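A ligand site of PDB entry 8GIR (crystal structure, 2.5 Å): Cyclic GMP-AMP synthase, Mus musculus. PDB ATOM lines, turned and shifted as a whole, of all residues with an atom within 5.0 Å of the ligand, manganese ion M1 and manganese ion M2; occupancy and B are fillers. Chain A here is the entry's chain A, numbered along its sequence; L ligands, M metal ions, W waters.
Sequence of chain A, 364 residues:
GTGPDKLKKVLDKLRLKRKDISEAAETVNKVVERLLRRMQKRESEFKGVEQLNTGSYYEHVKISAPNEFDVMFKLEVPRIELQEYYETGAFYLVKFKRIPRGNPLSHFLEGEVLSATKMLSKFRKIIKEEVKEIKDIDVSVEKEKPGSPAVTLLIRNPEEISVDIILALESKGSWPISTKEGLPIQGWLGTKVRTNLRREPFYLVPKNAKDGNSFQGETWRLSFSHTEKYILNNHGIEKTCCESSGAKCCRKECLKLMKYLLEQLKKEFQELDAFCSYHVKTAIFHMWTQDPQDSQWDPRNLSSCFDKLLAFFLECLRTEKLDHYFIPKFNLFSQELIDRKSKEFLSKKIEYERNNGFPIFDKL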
ATOM      1  N   GLY A  55     -17.646  30.231  -2.935  1.00  0.00           N
ATOM      2  CA  GLY A  55     -17.730  29.068  -3.794  1.00  0.00           C
ATOM      3  C   GLY A  55     -17.167  27.833  -3.120  1.00  0.00           C
ATOM      4  O   GLY A  55     -16.734  27.846  -1.965  1.00  0.00           O
ATOM      5  N   SER A  56     -17.180  26.741  -3.886  1.00  0.00           N
ATOM      6  CA  SER A  56     -17.045  25.430  -3.288  1.00  0.00           C
ATOM      7  C   SER A  56     -15.672  25.248  -2.679  1.00  0.00           C
ATOM      8  O   SER A  56     -15.541  24.567  -1.638  1.00  0.00           O
ATOM      9  CB  SER A  56     -17.325  24.339  -4.320  1.00  0.00           C
ATOM     10  OG  SER A  56     -16.422  24.417  -5.421  1.00  0.00           O
ATOM     11  N   GLU A  59     -15.679  26.779   0.698  1.00  0.00           N
ATOM     12  CA  GLU A  59     -16.617  26.020   1.526  1.00  0.00           C
ATOM     13  C   GLU A  59     -16.124  24.605   1.815  1.00  0.00           C
ATOM     14  O   GLU A  59     -16.760  23.885   2.605  1.00  0.00           O
ATOM     15  CB  GLU A  59     -18.008  25.979   0.860  1.00  0.00           C
ATOM     16  CG  GLU A  59     -18.701  27.343   0.705  1.00  0.00           C
ATOM     17  CD  GLU A  59     -19.735  27.355  -0.410  1.00  0.00           C
ATOM     18  OE1 GLU A  59     -19.804  26.354  -1.149  1.00  0.00           O
ATOM     19  OE2 GLU A  59     -20.503  28.343  -0.570  1.00  0.00           O
ATOM     20  N   LYS A  62     -15.375  21.607  -2.900  1.00  0.00           N
ATOM     21  CA  LYS A  62     -14.809  21.414  -4.220  1.00  0.00           C
ATOM     22  C   LYS A  62     -14.346  19.969  -4.365  1.00  0.00           C
ATOM     23  O   LYS A  62     -13.747  19.419  -3.448  1.00  0.00           O
ATOM     24  CB  LYS A  62     -13.628  22.370  -4.408  1.00  0.00           C
ATOM     25  CG  LYS A  62     -12.971  22.360  -5.732  1.00  0.00           C
ATOM     26  CD  LYS A  62     -13.914  22.650  -6.840  1.00  0.00           C
ATOM     27  CE  LYS A  62     -13.125  22.679  -8.119  1.00  0.00           C
ATOM     28  NZ  LYS A  62     -13.528  21.633  -9.076  1.00  0.00           N
ATOM     29  N   GLU A  68     -11.088  25.136  -9.982  1.00  0.00           N
ATOM     30  CA  GLU A  68     -12.047  26.210 -10.210  1.00  0.00           C
ATOM     31  C   GLU A  68     -12.246  26.973  -8.914  1.00  0.00           C
ATOM     32  O   GLU A  68     -12.691  26.381  -7.937  1.00  0.00           O
ATOM     33  CB  GLU A  68     -13.367  25.672 -10.728  1.00  0.00           C
ATOM     34  CG  GLU A  68     -14.121  26.655 -11.580  1.00  0.00           C
ATOM     35  CD  GLU A  68     -15.048  27.549 -10.776  1.00  0.00           C
ATOM     36  OE1 GLU A  68     -15.162  27.347  -9.572  1.00  0.00           O
ATOM     37  OE2 GLU A  68     -15.661  28.467 -11.360  1.00  0.00           O
ATOM     38  N   ASP A  70     -13.631  30.752  -7.016  1.00  0.00           N
ATOM     39  CA  ASP A  70     -14.528  31.897  -7.202  1.00  0.00           C
ATOM     40  C   ASP A  70     -14.198  32.999  -6.208  1.00  0.00           C
ATOM     41  O   ASP A  70     -14.052  32.729  -5.008  1.00  0.00           O
ATOM     42  CB  ASP A  70     -15.998  31.498  -7.069  1.00  0.00           C
ATOM     43  CG  ASP A  70     -16.331  30.270  -7.849  1.00  0.00           C
ATOM     44  OD1 ASP A  70     -16.367  30.337  -9.107  1.00  0.00           O
ATOM     45  OD2 ASP A  70     -16.544  29.227  -7.213  1.00  0.00           O
ATOM     46  N   ASP A 164     -13.094  32.603 -11.481  1.00  0.00           N
ATOM     47  CA  ASP A 164     -14.128  33.565 -11.794  1.00  0.00           C
ATOM     48  C   ASP A 164     -13.943  34.804 -10.935  1.00  0.00           C
ATOM     49  O   ASP A 164     -14.058  34.722  -9.710  1.00  0.00           O
ATOM     50  CB  ASP A 164     -15.514  32.968 -11.519  1.00  0.00           C
ATOM     51  CG  ASP A 164     -15.870  31.875 -12.482  1.00  0.00           C
ATOM     52  OD1 ASP A 164     -15.249  31.783 -13.574  1.00  0.00           O
ATOM     53  OD2 ASP A 164     -16.773  31.098 -12.143  1.00  0.00           O
ATOM     54  N   ARG A 221     -28.412  41.256 -10.209  1.00  0.00           N
ATOM     55  CA  ARG A 221     -28.949  40.066  -9.555  1.00  0.00           C
ATOM     56  C   ARG A 221     -28.366  39.923  -8.153  1.00  0.00           C
ATOM     57  O   ARG A 221     -27.143  40.058  -7.960  1.00  0.00           O
ATOM     58  CB  ARG A 221     -28.656  38.800 -10.378  1.00  0.00           C
ATOM     59  CG  ARG A 221     -29.346  37.541  -9.878  1.00  0.00           C
ATOM     60  CD  ARG A 221     -28.537  36.293 -10.249  1.00  0.00           C
ATOM     61  NE  ARG A 221     -27.583  35.997  -9.185  1.00  0.00           N
ATOM     62  CZ  ARG A 221     -26.360  35.506  -9.383  1.00  0.00           C
ATOM     63  NH1 ARG A 221     -25.909  35.226 -10.596  1.00  0.00           N
ATOM     64  NH2 ARG A 221     -25.572  35.290  -8.324  1.00  0.00           N
ATOM     65  N   PHE A 224     -25.907  35.894  -2.586  1.00  0.00           N
ATOM     66  CA  PHE A 224     -25.737  35.540  -1.177  1.00  0.00           C
ATOM     67  C   PHE A 224     -24.596  34.551  -0.992  1.00  0.00           C
ATOM     68  O   PHE A 224     -24.639  33.712  -0.092  1.00  0.00           O
ATOM     69  CB  PHE A 224     -27.057  34.996  -0.624  1.00  0.00           C
ATOM     70  CG  PHE A 224     -28.140  36.028  -0.586  1.00  0.00           C
ATOM     71  CD1 PHE A 224     -28.177  36.960   0.436  1.00  0.00           C
ATOM     72  CD2 PHE A 224     -29.045  36.116  -1.610  1.00  0.00           C
ATOM     73  CE1 PHE A 224     -29.125  37.946   0.463  1.00  0.00           C
ATOM     74  CE2 PHE A 224     -30.028  37.114  -1.603  1.00  0.00           C
ATOM     75  CZ  PHE A 224     -30.066  38.040  -0.565  1.00  0.00           C
ATOM     76  N   SER A 225     -23.569  34.632  -1.850  1.00  0.00           N
ATOM     77  CA  SER A 225     -22.446  33.723  -1.699  1.00  0.00           C
ATOM     78  C   SER A 225     -21.846  33.826  -0.324  1.00  0.00           C
ATOM     79  O   SER A 225     -21.445  32.816   0.259  1.00  0.00           O
ATOM     80  CB  SER A 225     -21.365  33.995  -2.732  1.00  0.00           C
ATOM     81  OG  SER A 225     -21.886  33.721  -3.999  1.00  0.00           O
ATOM     82  N   GLU A 228     -24.015  31.875   2.060  1.00  0.00           N
ATOM     83  CA  GLU A 228     -23.862  30.454   1.826  1.00  0.00           C
ATOM     84  C   GLU A 228     -22.546  29.922   2.386  1.00  0.00           C
ATOM     85  O   GLU A 228     -22.490  28.822   2.949  1.00  0.00           O
ATOM     86  CB  GLU A 228     -24.006  30.168   0.331  1.00  0.00           C
ATOM     87  CG  GLU A 228     -25.358  30.669  -0.196  1.00  0.00           C
ATOM     88  CD  GLU A 228     -25.391  30.738  -1.703  1.00  0.00           C
ATOM     89  OE1 GLU A 228     -24.436  30.245  -2.318  1.00  0.00           O
ATOM     90  OE2 GLU A 228     -26.375  31.255  -2.273  1.00  0.00           O
ATOM     91  N   LYS A 259     -23.020  16.767  -6.097  1.00  0.00           N
ATOM     92  CA  LYS A 259     -22.265  17.555  -7.063  1.00  0.00           C
ATOM     93  C   LYS A 259     -21.652  16.658  -8.112  1.00  0.00           C
ATOM     94  O   LYS A 259     -21.734  16.930  -9.322  1.00  0.00           O
ATOM     95  CB  LYS A 259     -21.162  18.350  -6.351  1.00  0.00           C
ATOM     96  CG  LYS A 259     -21.636  19.579  -5.612  1.00  0.00           C
ATOM     97  CD  LYS A 259     -20.560  20.052  -4.653  1.00  0.00           C
ATOM     98  CE  LYS A 259     -19.335  20.549  -5.386  1.00  0.00           C
ATOM     99  NZ  LYS A 259     -19.657  21.782  -6.103  1.00  0.00           N
ATOM    100  N   GLU A 263     -22.008  16.607 -12.122  1.00  0.00           N
ATOM    101  CA  GLU A 263     -20.812  16.832 -12.945  1.00  0.00           C
ATOM    102  C   GLU A 263     -20.599  15.731 -13.983  1.00  0.00           C
ATOM    103  O   GLU A 263     -20.400  16.011 -15.170  1.00  0.00           O
ATOM    104  CB  GLU A 263     -19.571  16.958 -12.054  1.00  0.00           C
ATOM    105  CG  GLU A 263     -19.318  18.354 -11.519  1.00  0.00           C
ATOM    106  CD  GLU A 263     -17.965  18.505 -10.810  1.00  0.00           C
ATOM    107  OE1 GLU A 263     -17.001  17.818 -11.230  1.00  0.00           O
ATOM    108  OE2 GLU A 263     -17.882  19.318  -9.848  1.00  0.00           O
ATOM    109  N   CYS A 276     -26.889  23.284 -13.286  1.00  0.00           N
ATOM    110  CA  CYS A 276     -25.622  23.760 -12.756  1.00  0.00           C
ATOM    111  C   CYS A 276     -25.547  23.350 -11.301  1.00  0.00           C
ATOM    112  O   CYS A 276     -26.556  23.030 -10.669  1.00  0.00           O
ATOM    113  CB  CYS A 276     -25.478  25.285 -12.934  1.00  0.00           C
ATOM    114  SG  CYS A 276     -26.570  26.266 -11.875  1.00  0.00           S
ATOM    115  N   SER A 277     -24.346  23.418 -10.750  1.00  0.00           N
ATOM    116  CA  SER A 277     -24.143  22.930  -9.401  1.00  0.00           C
ATOM    117  C   SER A 277     -24.898  23.748  -8.352  1.00  0.00           C
ATOM    118  O   SER A 277     -25.168  23.239  -7.256  1.00  0.00           O
ATOM    119  CB  SER A 277     -22.652  22.942  -9.100  1.00  0.00           C
ATOM    120  OG  SER A 277     -22.216  24.283  -8.923  1.00  0.00           O
ATOM    121  N   TYR A 278     -25.270  24.991  -8.641  1.00  0.00           N
ATOM    122  CA  TYR A 278     -26.049  25.753  -7.674  1.00  0.00           C
ATOM    123  C   TYR A 278     -27.415  25.140  -7.472  1.00  0.00           C
ATOM    124  O   TYR A 278     -28.030  25.345  -6.416  1.00  0.00           O
ATOM    125  CB  TYR A 278     -26.202  27.202  -8.121  1.00  0.00           C
ATOM    126  CG  TYR A 278     -26.759  28.132  -7.065  1.00  0.00           C
ATOM    127  CD1 TYR A 278     -26.005  28.462  -5.938  1.00  0.00           C
ATOM    128  CD2 TYR A 278     -28.045  28.706  -7.187  1.00  0.00           C
ATOM    129  CE1 TYR A 278     -26.500  29.332  -4.952  1.00  0.00           C
ATOM    130  CE2 TYR A 278     -28.541  29.576  -6.202  1.00  0.00           C
ATOM    131  CZ  TYR A 278     -27.755  29.876  -5.088  1.00  0.00           C
ATOM    132  OH  TYR A 278     -28.184  30.737  -4.103  1.00  0.00           O
ATOM    133  N   LYS A 281     -26.800  22.652  -4.773  1.00  0.00           N
ATOM    134  CA  LYS A 281     -26.536  23.383  -3.532  1.00  0.00           C
ATOM    135  C   LYS A 281     -27.838  23.911  -2.945  1.00  0.00           C
ATOM    136  O   LYS A 281     -28.064  23.800  -1.727  1.00  0.00           O
ATOM    137  CB  LYS A 281     -25.574  24.542  -3.785  1.00  0.00           C
ATOM    138  CG  LYS A 281     -25.067  25.238  -2.537  1.00  0.00           C
ATOM    139  CD  LYS A 281     -24.258  26.467  -2.889  1.00  0.00           C
ATOM    140  CE  LYS A 281     -23.231  26.794  -1.794  1.00  0.00           C
ATOM    141  NZ  LYS A 281     -22.563  28.137  -2.015  1.00  0.00           N
ATOM    142  N   HIS A 324     -35.488  29.294  -4.909  1.00  0.00           N
ATOM    143  CA  HIS A 324     -34.269  29.918  -4.422  1.00  0.00           C
ATOM    144  C   HIS A 324     -34.321  29.996  -2.902  1.00  0.00           C
ATOM    145  O   HIS A 324     -35.344  30.386  -2.330  1.00  0.00           O
ATOM    146  CB  HIS A 324     -34.146  31.304  -5.044  1.00  0.00           C
ATOM    147  CG  HIS A 324     -32.819  31.941  -4.874  1.00  0.00           C
ATOM    148  ND1 HIS A 324     -32.322  32.331  -3.639  1.00  0.00           N
ATOM    149  CD2 HIS A 324     -31.884  32.318  -5.774  1.00  0.00           C
ATOM    150  CE1 HIS A 324     -31.134  32.882  -3.795  1.00  0.00           C
ATOM    151  NE2 HIS A 324     -30.846  32.888  -5.083  1.00  0.00           N
HETATM  152  P1  LIG L   1     -18.483  24.197  -8.187  1.00  0.00           P
HETATM  153  O1  LIG L   1     -19.383  23.507  -9.174  1.00  0.00           O
HETATM  154  O2  LIG L   1     -17.525  23.290  -7.452  1.00  0.00           O
HETATM  155  O3  LIG L   1     -17.721  25.318  -8.868  1.00  0.00           O
HETATM  156  P2  LIG L   1     -19.704  26.410  -6.621  1.00  0.00           P
HETATM  157  O4  LIG L   1     -20.751  26.575  -5.595  1.00  0.00           O
HETATM  158  O5  LIG L   1     -18.409  27.132  -6.360  1.00  0.00           O
HETATM  159  O6  LIG L   1     -19.316  24.941  -7.041  1.00  0.00           O
HETATM  160  P3  LIG L   1     -19.954  28.089  -9.039  1.00  0.00           P
HETATM  161  O7  LIG L   1     -20.802  27.782 -10.208  1.00  0.00           O
HETATM  162  O8  LIG L   1     -18.442  28.062  -9.156  1.00  0.00           O
HETATM  163  O9  LIG L   1     -20.289  26.946  -8.003  1.00  0.00           O
HETATM  164  O10 LIG L   1     -20.447  29.470  -8.449  1.00  0.00           O
HETATM  165  C1  LIG L   1     -19.826  30.056  -7.284  1.00  0.00           C
HETATM  166  C2  LIG L   1     -20.879  30.601  -6.344  1.00  0.00           C
HETATM  167  O11 LIG L   1     -21.651  31.635  -6.992  1.00  0.00           O
HETATM  168  C3  LIG L   1     -21.920  29.620  -5.816  1.00  0.00           C
HETATM  169  O12 LIG L   1     -21.420  28.937  -4.670  1.00  0.00           O
HETATM  170  C4  LIG L   1     -23.071  30.556  -5.437  1.00  0.00           C
HETATM  171  O13 LIG L   1     -22.828  31.247  -4.214  1.00  0.00           O
HETATM  172  C5  LIG L   1     -23.002  31.587  -6.558  1.00  0.00           C
HETATM  173  N1  LIG L   1     -23.834  31.243  -7.708  1.00  0.00           N
HETATM  174  C6  LIG L   1     -23.490  30.495  -8.810  1.00  0.00           C
HETATM  175  N2  LIG L   1     -24.461  30.337  -9.676  1.00  0.00           N
HETATM  176  C7  LIG L   1     -25.527  31.023  -9.095  1.00  0.00           C
HETATM  177  C8  LIG L   1     -26.851  31.253  -9.517  1.00  0.00           C
HETATM  178  N3  LIG L   1     -27.362  30.777 -10.668  1.00  0.00           N
HETATM  179  N4  LIG L   1     -27.645  32.001  -8.719  1.00  0.00           N
HETATM  180  C9  LIG L   1     -27.150  32.461  -7.571  1.00  0.00           C
HETATM  181  N5  LIG L   1     -25.929  32.303  -7.060  1.00  0.00           N
HETATM  182  C10 LIG L   1     -25.155  31.580  -7.889  1.00  0.00           C
HETATM  183 MN    MN M   1     -16.781  27.011  -7.981  1.00  0.00          MN
HETATM  184 MN    MN M   2     -17.698  29.570 -10.918  1.00  0.00          MN
HETATM  185  O   HOH W   1     -20.523  25.202  -3.312  1.00  0.00           O
HETATM  186  O   HOH W   2     -30.267  33.238  -9.067  1.00  0.00           O
HETATM  187  O   HOH W   3     -19.203  31.290 -10.809  1.00  0.00           O
HETATM  188  O   HOH W   4     -22.949  25.403  -6.452  1.00  0.00           O
HETATM  189  O   HOH W   5     -26.283  33.306  -4.252  1.00  0.00           O
HETATM  190  O   HOH W   6     -23.517  26.349 -10.524  1.00  0.00           O
HETATM  191  O   HOH W   7     -16.348  20.778  -7.843  1.00  0.00           O
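The backbone carbonyl oxygen of Ser 56 lies within hydrogen-bond range of the backbone NH of Lys 62, at 3.2 Å.
OE1 of Glu 228 is in salt-bridge range of NZ of Lys 281 (2.8 Å).
N of Tyr 278 lies close to SG of Cys 276 (3.7 Å).
The side-chain carboxylate of Glu 228 lies within hydrogen-bond range of the side-chain hydroxyl of Tyr 278, at 2.6 Å.
The side-chain amino group (NZ) of Lys 281 is in salt-bridge range of the side-chain carboxylate (OE2) of Glu 59 (2.5 Å).
Manganese ion M1 is bound by an oxygen (O3) of the ligand (2.1 Å), an oxygen (O8) of the ligand (2.3 Å), the side-chain carboxylate (OE1) of Glu 68 (2.3 Å), an oxygen (O5) of the ligand (2.3 Å) and the side-chain carboxylate (OD2) of Asp 70 (2.4 Å).
Manganese ion M1 has five donor atoms within binding distance.
NH2 of Arg 221 sits at hydrogen-bond distance from N5 of the ligand.
The side-chain hydroxyl of Ser 277 lies within hydrogen-bond range of an oxygen (O1) of the ligand (2.9 Å).
The backbone NH (N) of Ser 56 lies close to an oxygen (O5) of the ligand.
O13 of the ligand lies within hydrogen-bond range of OG of Ser 225 (2.7 Å).
An oxygen (O12) of the ligand is in hydrogen-bond range of the side-chain amino group of Lys 281 (3.0 Å).
An oxygen (O2) of the ligand is in salt-bridge range of the side-chain amino group of Lys 259 (2.9 Å).
The side-chain hydroxyl (OG) of Ser 56 lies within hydrogen-bond range of an oxygen (O2) of the ligand.
O13 of the ligand sits at hydrogen-bond distance from OE1 of Glu 228 (2.7 Å).
Manganese ion M2 is bound by OD2 of Asp 164 (2.2 Å), water W3 (2.3 Å), OE2 of Glu 68 (2.4 Å), OD1 of Asp 70 (2.4 Å) and O8 of the ligand (2.4 Å).
Ser 56 touches manganese ion M1.
Three residues have an atom within 4 Å of manganese ion M1: Ser 56, Glu 68 and Asp 70.
Within 4 Å of manganese ion M2: Glu 68, Asp 70 and Asp 164.
The nearest printed residue that does not touch manganese ion M2 is Gly 55 (7.1 Å).
Gly 55 touches the ligand.
Lys 62 touches the ligand (CD to O2, 3.7 Å).
Tyr 278 touches the ligand.
Hydrophobic or aromatic side chains within 4 Å of the ligand: Tyr 278.
Of the 18 residues printed, 12 come within 4 Å of the ligand.
The nearest printed residue that does not touch the ligand is Glu 59 (4.2 Å).
Water W4 lies within hydrogen-bond range of O4 of the ligand (2.6 Å), OG of Ser 277 (2.8 Å) and N of Tyr 278 (3.2 Å).
Water W1 bridges the side-chain carboxylate of Glu 59 (2.6 Å) and an oxygen (O4) of the ligand (2.7 Å).
Water W7 lies within hydrogen-bond range of an oxygen (O2) of the ligand, the side-chain carboxylate (OE2) of Glu 263 and the side-chain amino group (NZ) of Lys 62.
Water W5 lies within hydrogen-bond range of OE2 of Glu 228 (2.9 Å), N5 of the ligand (3.0 Å), N of Phe 224 (3.1 Å) and OH of Tyr 278 (3.2 Å).
Water W6 lies within hydrogen-bond range of N of Tyr 278 (2.9 Å), OG of Ser 277 (2.9 Å), O7 of the ligand (3.1 Å) and SG of Cys 276 (3.3 Å).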
